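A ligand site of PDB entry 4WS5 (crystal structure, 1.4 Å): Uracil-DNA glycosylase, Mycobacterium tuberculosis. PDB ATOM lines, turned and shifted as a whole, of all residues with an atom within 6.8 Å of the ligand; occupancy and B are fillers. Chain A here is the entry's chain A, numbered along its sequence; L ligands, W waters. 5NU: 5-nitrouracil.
Water W2 lies within hydrogen-bond range of O53 of the ligand (2.4 Å) and OG of Ser 104 (2.7 Å).
Water W3 bridges O4 of the ligand (2.7 Å) and NE2 of His 202 (2.9 Å).
Water W1 bridges an oxygen (O2) of the ligand (2.7 Å) and the backbone NH of Tyr 81 (3.0 Å).
OD1 of Asn 138 sits at hydrogen-bond distance from N3 of the ligand, 2.8 Å away.
The backbone NH of Gln 78 sits at hydrogen-bond distance from an oxygen (O4) of the ligand (2.8 Å).
O of Asp 79 sits at hydrogen-bond distance from N3 of the ligand (3.0 Å).
A ring nitrogen (NE2) of His 202 sits at hydrogen-bond distance from an oxygen (O52) of the ligand (3.0 Å).
The backbone NH (N) of Phe 92 is in hydrogen-bond range of an oxygen (O2) of the ligand (3.0 Å).
An oxygen (O53) of the ligand lies within hydrogen-bond range of the side-chain hydroxyl of Ser 104 (3.2 Å).
Residues that only touch the ligand: Ser 91 (3.3 Å), Gly 77 (3.5 Å) and Tyr 81 (3.5 Å).
Nine residues have an atom within 4 Å of the ligand: Gly 77, Gln 78, Asp 79, Tyr 81, Ser 91, Phe 92, Ser 104, Asn 138 and His 202.
OD1 of Asn 138 sits at hydrogen-bond distance from N of Gln 78 (3.2 Å).
A ring nitrogen (ND1) of His 202 lies within hydrogen-bond range of the backbone NH (N) of Ser 204.
The backbone carbonyl oxygen (O) of Phe 92 sits at hydrogen-bond distance from the side-chain hydroxyl (OH) of Tyr 81 (2.7 Å).
The side-chain hydroxyl (OG) of Ser 91 sits at hydrogen-bond distance from the backbone NH (N) of Leu 137 (3.3 Å).
The backbone NH (N) of Ser 91 lies within hydrogen-bond range of the backbone carbonyl oxygen (O) of Leu 136, 2.9 Å away.
The backbone NH (N) of Gly 77 is in hydrogen-bond range of the backbone carbonyl oxygen (O) of Leu 137, at 2.9 Å.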
ATOM      1  N   VAL A  76     -18.148 -24.496  19.993  1.00  0.00           N
ATOM      2  CA  VAL A  76     -16.806 -24.321  20.516  1.00  0.00           C
ATOM      3  C   VAL A  76     -15.768 -24.508  19.423  1.00  0.00           C
ATOM      4  O   VAL A  76     -15.775 -25.483  18.712  1.00  0.00           O
ATOM      5  CB  VAL A  76     -16.523 -25.366  21.660  1.00  0.00           C
ATOM      6  CG1 VAL A  76     -15.125 -25.238  22.178  1.00  0.00           C
ATOM      7  CG2 VAL A  76     -17.516 -25.199  22.783  1.00  0.00           C
ATOM      8  N   GLY A  77     -14.847 -23.573  19.357  1.00  0.00           N
ATOM      9  CA  GLY A  77     -13.602 -23.693  18.601  1.00  0.00           C
ATOM     10  C   GLY A  77     -12.428 -23.799  19.541  1.00  0.00           C
ATOM     11  O   GLY A  77     -12.570 -23.584  20.776  1.00  0.00           O
ATOM     12  N   GLN A  78     -11.290 -24.012  18.948  1.00  0.00           N
ATOM     13  CA  GLN A  78     -10.075 -24.160  19.716  1.00  0.00           C
ATOM     14  C   GLN A  78      -9.233 -22.889  19.720  1.00  0.00           C
ATOM     15  O   GLN A  78      -9.002 -22.279  20.756  1.00  0.00           O
ATOM     16  CB  GLN A  78      -9.324 -25.417  19.326  1.00  0.00           C
ATOM     17  CG  GLN A  78     -10.139 -26.662  19.660  1.00  0.00           C
ATOM     18  CD  GLN A  78     -10.429 -26.747  21.184  1.00  0.00           C
ATOM     19  OE1 GLN A  78      -9.593 -26.410  22.046  1.00  0.00           O
ATOM     20  NE2 GLN A  78     -11.638 -27.179  21.549  1.00  0.00           N
ATOM     21  N   ASP A  79      -8.717 -22.506  18.553  1.00  0.00           N
ATOM     22  CA  ASP A  79      -7.899 -21.326  18.413  1.00  0.00           C
ATOM     23  C   ASP A  79      -8.391 -20.555  17.178  1.00  0.00           C
ATOM     24  O   ASP A  79      -8.947 -21.167  16.257  1.00  0.00           O
ATOM     25  CB  ASP A  79      -6.395 -21.748  18.142  1.00  0.00           C
ATOM     26  CG  ASP A  79      -5.806 -22.549  19.254  1.00  0.00           C
ATOM     27  OD1 ASP A  79      -5.986 -23.817  19.277  1.00  0.00           O
ATOM     28  OD2 ASP A  79      -5.207 -21.984  20.168  1.00  0.00           O
ATOM     29  N   PRO A  80      -8.094 -19.281  17.099  1.00  0.00           N
ATOM     30  CA  PRO A  80      -8.475 -18.557  15.877  1.00  0.00           C
ATOM     31  C   PRO A  80      -7.718 -18.998  14.647  1.00  0.00           C
ATOM     32  O   PRO A  80      -6.602 -19.534  14.775  1.00  0.00           O
ATOM     33  CB  PRO A  80      -8.172 -17.087  16.209  1.00  0.00           C
ATOM     34  CG  PRO A  80      -7.998 -17.071  17.716  1.00  0.00           C
ATOM     35  CD  PRO A  80      -7.437 -18.395  18.075  1.00  0.00           C
ATOM     36  N   TYR A  81      -8.280 -18.773  13.475  1.00  0.00           N
ATOM     37  CA  TYR A  81      -7.543 -19.059  12.269  1.00  0.00           C
ATOM     38  C   TYR A  81      -6.177 -18.344  12.335  1.00  0.00           C
ATOM     39  O   TYR A  81      -6.102 -17.173  12.689  1.00  0.00           O
ATOM     40  CB  TYR A  81      -8.246 -18.501  11.014  1.00  0.00           C
ATOM     41  CG  TYR A  81      -9.522 -19.163  10.657  1.00  0.00           C
ATOM     42  CD1 TYR A  81      -9.547 -20.477  10.272  1.00  0.00           C
ATOM     43  CD2 TYR A  81     -10.759 -18.467  10.651  1.00  0.00           C
ATOM     44  CE1 TYR A  81     -10.721 -21.088   9.912  1.00  0.00           C
ATOM     45  CE2 TYR A  81     -11.928 -19.053  10.267  1.00  0.00           C
ATOM     46  CZ  TYR A  81     -11.921 -20.387   9.900  1.00  0.00           C
ATOM     47  OH  TYR A  81     -13.066 -21.058   9.483  1.00  0.00           O
ATOM     48  N   ALA A  87      -9.234 -14.586  10.849  1.00  0.00           N
ATOM     49  CA  ALA A  87      -9.906 -14.505  12.146  1.00  0.00           C
ATOM     50  C   ALA A  87     -10.621 -13.181  12.368  1.00  0.00           C
ATOM     51  O   ALA A  87      -9.985 -12.113  12.177  1.00  0.00           O
ATOM     52  CB  ALA A  87      -8.970 -14.738  13.305  1.00  0.00           C
ATOM     53  N   LEU A  90     -15.080 -14.458  16.003  1.00  0.00           N
ATOM     54  CA  LEU A  90     -16.157 -15.445  16.145  1.00  0.00           C
ATOM     55  C   LEU A  90     -15.626 -16.726  15.552  1.00  0.00           C
ATOM     56  O   LEU A  90     -15.062 -16.737  14.452  1.00  0.00           O
ATOM     57  CB  LEU A  90     -17.360 -15.013  15.315  1.00  0.00           C
ATOM     58  CG  LEU A  90     -18.053 -13.746  15.702  1.00  0.00           C
ATOM     59  CD1 LEU A  90     -19.211 -13.435  14.743  1.00  0.00           C
ATOM     60  CD2 LEU A  90     -18.593 -13.809  17.133  1.00  0.00           C
ATOM     61  N   SER A  91     -15.713 -17.822  16.300  1.00  0.00           N
ATOM     62  CA  SER A  91     -15.120 -19.068  15.823  1.00  0.00           C
ATOM     63  C   SER A  91     -15.686 -19.413  14.420  1.00  0.00           C
ATOM     64  O   SER A  91     -16.891 -19.222  14.148  1.00  0.00           O
ATOM     65  CB  SER A  91     -15.377 -20.176  16.875  1.00  0.00           C
ATOM     66  OG  SER A  91     -16.701 -20.435  17.052  1.00  0.00           O
ATOM     67  N   PHE A  92     -14.795 -19.826  13.534  1.00  0.00           N
ATOM     68  CA  PHE A  92     -15.070 -20.325  12.208  1.00  0.00           C
ATOM     69  C   PHE A  92     -15.399 -19.261  11.178  1.00  0.00           C
ATOM     70  O   PHE A  92     -15.208 -19.500   9.995  1.00  0.00           O
ATOM     71  CB  PHE A  92     -16.143 -21.419  12.204  1.00  0.00           C
ATOM     72  CG  PHE A  92     -15.777 -22.625  13.057  1.00  0.00           C
ATOM     73  CD1 PHE A  92     -14.840 -23.536  12.602  1.00  0.00           C
ATOM     74  CD2 PHE A  92     -16.331 -22.789  14.329  1.00  0.00           C
ATOM     75  CE1 PHE A  92     -14.518 -24.634  13.340  1.00  0.00           C
ATOM     76  CE2 PHE A  92     -15.906 -23.853  15.149  1.00  0.00           C
ATOM     77  CZ  PHE A  92     -15.018 -24.739  14.600  1.00  0.00           C
ATOM     78  N   SER A  93     -15.881 -18.120  11.615  1.00  0.00           N
ATOM     79  CA  SER A  93     -16.313 -17.064  10.693  1.00  0.00           C
ATOM     80  C   SER A  93     -15.153 -16.396   9.958  1.00  0.00           C
ATOM     81  O   SER A  93     -14.030 -16.324  10.484  1.00  0.00           O
ATOM     82  CB  SER A  93     -17.086 -16.038  11.504  1.00  0.00           C
ATOM     83  OG  SER A  93     -17.768 -15.095  10.694  1.00  0.00           O
ATOM     84  N   PRO A 102     -11.955 -20.894   4.265  1.00  0.00           N
ATOM     85  CA  PRO A 102     -11.166 -21.923   4.920  1.00  0.00           C
ATOM     86  C   PRO A 102     -11.850 -23.276   4.758  1.00  0.00           C
ATOM     87  O   PRO A 102     -13.090 -23.375   4.791  1.00  0.00           O
ATOM     88  CB  PRO A 102     -11.174 -21.487   6.397  1.00  0.00           C
ATOM     89  CG  PRO A 102     -11.356 -20.003   6.347  1.00  0.00           C
ATOM     90  CD  PRO A 102     -12.282 -19.795   5.163  1.00  0.00           C
ATOM     91  N   SER A 104     -12.319 -25.875   6.640  1.00  0.00           N
ATOM     92  CA  SER A 104     -13.221 -26.295   7.704  1.00  0.00           C
ATOM     93  C   SER A 104     -14.595 -25.626   7.558  1.00  0.00           C
ATOM     94  O   SER A 104     -15.616 -26.231   7.783  1.00  0.00           O
ATOM     95  CB  SER A 104     -12.648 -26.032   9.090  1.00  0.00           C
ATOM     96  OG  SER A 104     -11.553 -26.917   9.370  1.00  0.00           O
ATOM     97  N   LEU A 105     -14.571 -24.318   7.259  1.00  0.00           N
ATOM     98  CA  LEU A 105     -15.780 -23.561   7.043  1.00  0.00           C
ATOM     99  C   LEU A 105     -16.535 -24.056   5.808  1.00  0.00           C
ATOM    100  O   LEU A 105     -17.746 -24.172   5.838  1.00  0.00           O
ATOM    101  CB  LEU A 105     -15.503 -22.088   6.941  1.00  0.00           C
ATOM    102  CG  LEU A 105     -16.716 -21.179   6.782  1.00  0.00           C
ATOM    103  CD1 LEU A 105     -17.614 -21.279   8.023  1.00  0.00           C
ATOM    104  CD2 LEU A 105     -16.286 -19.724   6.614  1.00  0.00           C
ATOM    105  N   ILE A 108     -18.261 -27.083   6.983  1.00  0.00           N
ATOM    106  CA  ILE A 108     -19.414 -26.679   7.760  1.00  0.00           C
ATOM    107  C   ILE A 108     -20.570 -26.283   6.850  1.00  0.00           C
ATOM    108  O   ILE A 108     -21.724 -26.699   7.047  1.00  0.00           O
ATOM    109  CB  ILE A 108     -19.074 -25.552   8.754  1.00  0.00           C
ATOM    110  CG1 ILE A 108     -18.166 -26.079   9.851  1.00  0.00           C
ATOM    111  CG2 ILE A 108     -20.332 -24.898   9.333  1.00  0.00           C
ATOM    112  CD1 ILE A 108     -17.435 -24.977  10.621  1.00  0.00           C
ATOM    113  N   LEU A 136     -20.168 -18.356  19.188  1.00  0.00           N
ATOM    114  CA  LEU A 136     -19.073 -18.887  18.350  1.00  0.00           C
ATOM    115  C   LEU A 136     -17.797 -18.600  19.133  1.00  0.00           C
ATOM    116  O   LEU A 136     -17.058 -17.642  18.862  1.00  0.00           O
ATOM    117  CB  LEU A 136     -19.127 -18.252  16.987  1.00  0.00           C
ATOM    118  CG  LEU A 136     -20.380 -18.638  16.172  1.00  0.00           C
ATOM    119  CD1 LEU A 136     -20.545 -17.648  15.044  1.00  0.00           C
ATOM    120  CD2 LEU A 136     -20.279 -20.044  15.645  1.00  0.00           C
ATOM    121  N   LEU A 137     -17.531 -19.462  20.102  1.00  0.00           N
ATOM    122  CA  LEU A 137     -16.502 -19.189  21.136  1.00  0.00           C
ATOM    123  C   LEU A 137     -15.307 -20.059  20.918  1.00  0.00           C
ATOM    124  O   LEU A 137     -15.404 -21.300  21.052  1.00  0.00           O
ATOM    125  CB  LEU A 137     -17.038 -19.449  22.548  1.00  0.00           C
ATOM    126  CG  LEU A 137     -16.088 -19.106  23.692  1.00  0.00           C
ATOM    127  CD1 LEU A 137     -15.665 -17.645  23.665  1.00  0.00           C
ATOM    128  CD2 LEU A 137     -16.700 -19.504  25.011  1.00  0.00           C
ATOM    129  N   ASN A 138     -14.120 -19.471  20.679  1.00  0.00           N
ATOM    130  CA  ASN A 138     -12.866 -20.216  20.747  1.00  0.00           C
ATOM    131  C   ASN A 138     -12.428 -20.324  22.190  1.00  0.00           C
ATOM    132  O   ASN A 138     -12.590 -19.403  23.007  1.00  0.00           O
ATOM    133  CB  ASN A 138     -11.782 -19.525  19.905  1.00  0.00           C
ATOM    134  CG  ASN A 138     -11.918 -19.863  18.453  1.00  0.00           C
ATOM    135  OD1 ASN A 138     -12.072 -21.037  18.098  1.00  0.00           O
ATOM    136  ND2 ASN A 138     -11.764 -18.898  17.571  1.00  0.00           N
ATOM    137  N   HIS A 202     -14.569 -33.513  13.874  1.00  0.00           N
ATOM    138  CA  HIS A 202     -14.394 -32.132  13.443  1.00  0.00           C
ATOM    139  C   HIS A 202     -14.649 -31.956  11.946  1.00  0.00           C
ATOM    140  O   HIS A 202     -14.384 -32.857  11.162  1.00  0.00           O
ATOM    141  CB  HIS A 202     -12.994 -31.725  13.868  1.00  0.00           C
ATOM    142  CG  HIS A 202     -12.707 -30.262  13.800  1.00  0.00           C
ATOM    143  ND1 HIS A 202     -12.346 -29.652  12.615  1.00  0.00           N
ATOM    144  CD2 HIS A 202     -12.632 -29.334  14.753  1.00  0.00           C
ATOM    145  CE1 HIS A 202     -12.119 -28.393  12.845  1.00  0.00           C
ATOM    146  NE2 HIS A 202     -12.306 -28.175  14.134  1.00  0.00           N
ATOM    147  N   PRO A 203     -15.089 -30.749  11.521  1.00  0.00           N
ATOM    148  CA  PRO A 203     -15.273 -30.517  10.087  1.00  0.00           C
ATOM    149  C   PRO A 203     -14.026 -30.357   9.238  1.00  0.00           C
ATOM    150  O   PRO A 203     -14.141 -30.249   8.017  1.00  0.00           O
ATOM    151  CB  PRO A 203     -16.113 -29.233  10.040  1.00  0.00           C
ATOM    152  CG  PRO A 203     -15.765 -28.518  11.353  1.00  0.00           C
ATOM    153  CD  PRO A 203     -15.627 -29.654  12.305  1.00  0.00           C
ATOM    154  N   SER A 204     -12.843 -30.322   9.830  1.00  0.00           N
ATOM    155  CA  SER A 204     -11.608 -30.297   9.031  1.00  0.00           C
ATOM    156  C   SER A 204     -11.607 -31.455   8.052  1.00  0.00           C
ATOM    157  O   SER A 204     -12.065 -32.543   8.375  1.00  0.00           O
ATOM    158  CB  SER A 204     -10.420 -30.477   9.963  1.00  0.00           C
ATOM    159  OG  SER A 204      -9.332 -30.886   9.331  1.00  0.00           O
HETATM  160  O4  5NU L   1     -11.140 -24.040  16.141  1.00  0.00           O
HETATM  161  C4  5NU L   1     -11.339 -23.267  15.185  1.00  0.00           C
HETATM  162  N3  5NU L   1     -11.676 -22.015  15.495  1.00  0.00           N
HETATM  163  C2  5NU L   1     -11.847 -21.110  14.522  1.00  0.00           C
HETATM  164  O2  5NU L   1     -12.118 -19.917  14.851  1.00  0.00           O
HETATM  165  N1  5NU L   1     -11.839 -21.401  13.259  1.00  0.00           N
HETATM  166  C6  5NU L   1     -11.583 -22.650  12.926  1.00  0.00           C
HETATM  167  C5  5NU L   1     -11.263 -23.630  13.841  1.00  0.00           C
HETATM  168  N51 5NU L   1     -11.003 -24.929  13.373  1.00  0.00           N
HETATM  169  O53 5NU L   1     -11.226 -25.247  12.028  1.00  0.00           O
HETATM  170  O52 5NU L   1     -10.537 -25.784  14.208  1.00  0.00           O
HETATM  171  O   HOH W   1     -10.997 -17.608  13.920  1.00  0.00           O
HETATM  172  O   HOH W   2      -9.562 -26.843  11.224  1.00  0.00           O
HETATM  173  O   HOH W   3     -11.889 -26.630  16.558  1.00  0.00           O
HETATM  174  O   HOH W   4      -7.894 -22.778  14.126  1.00  0.00           O
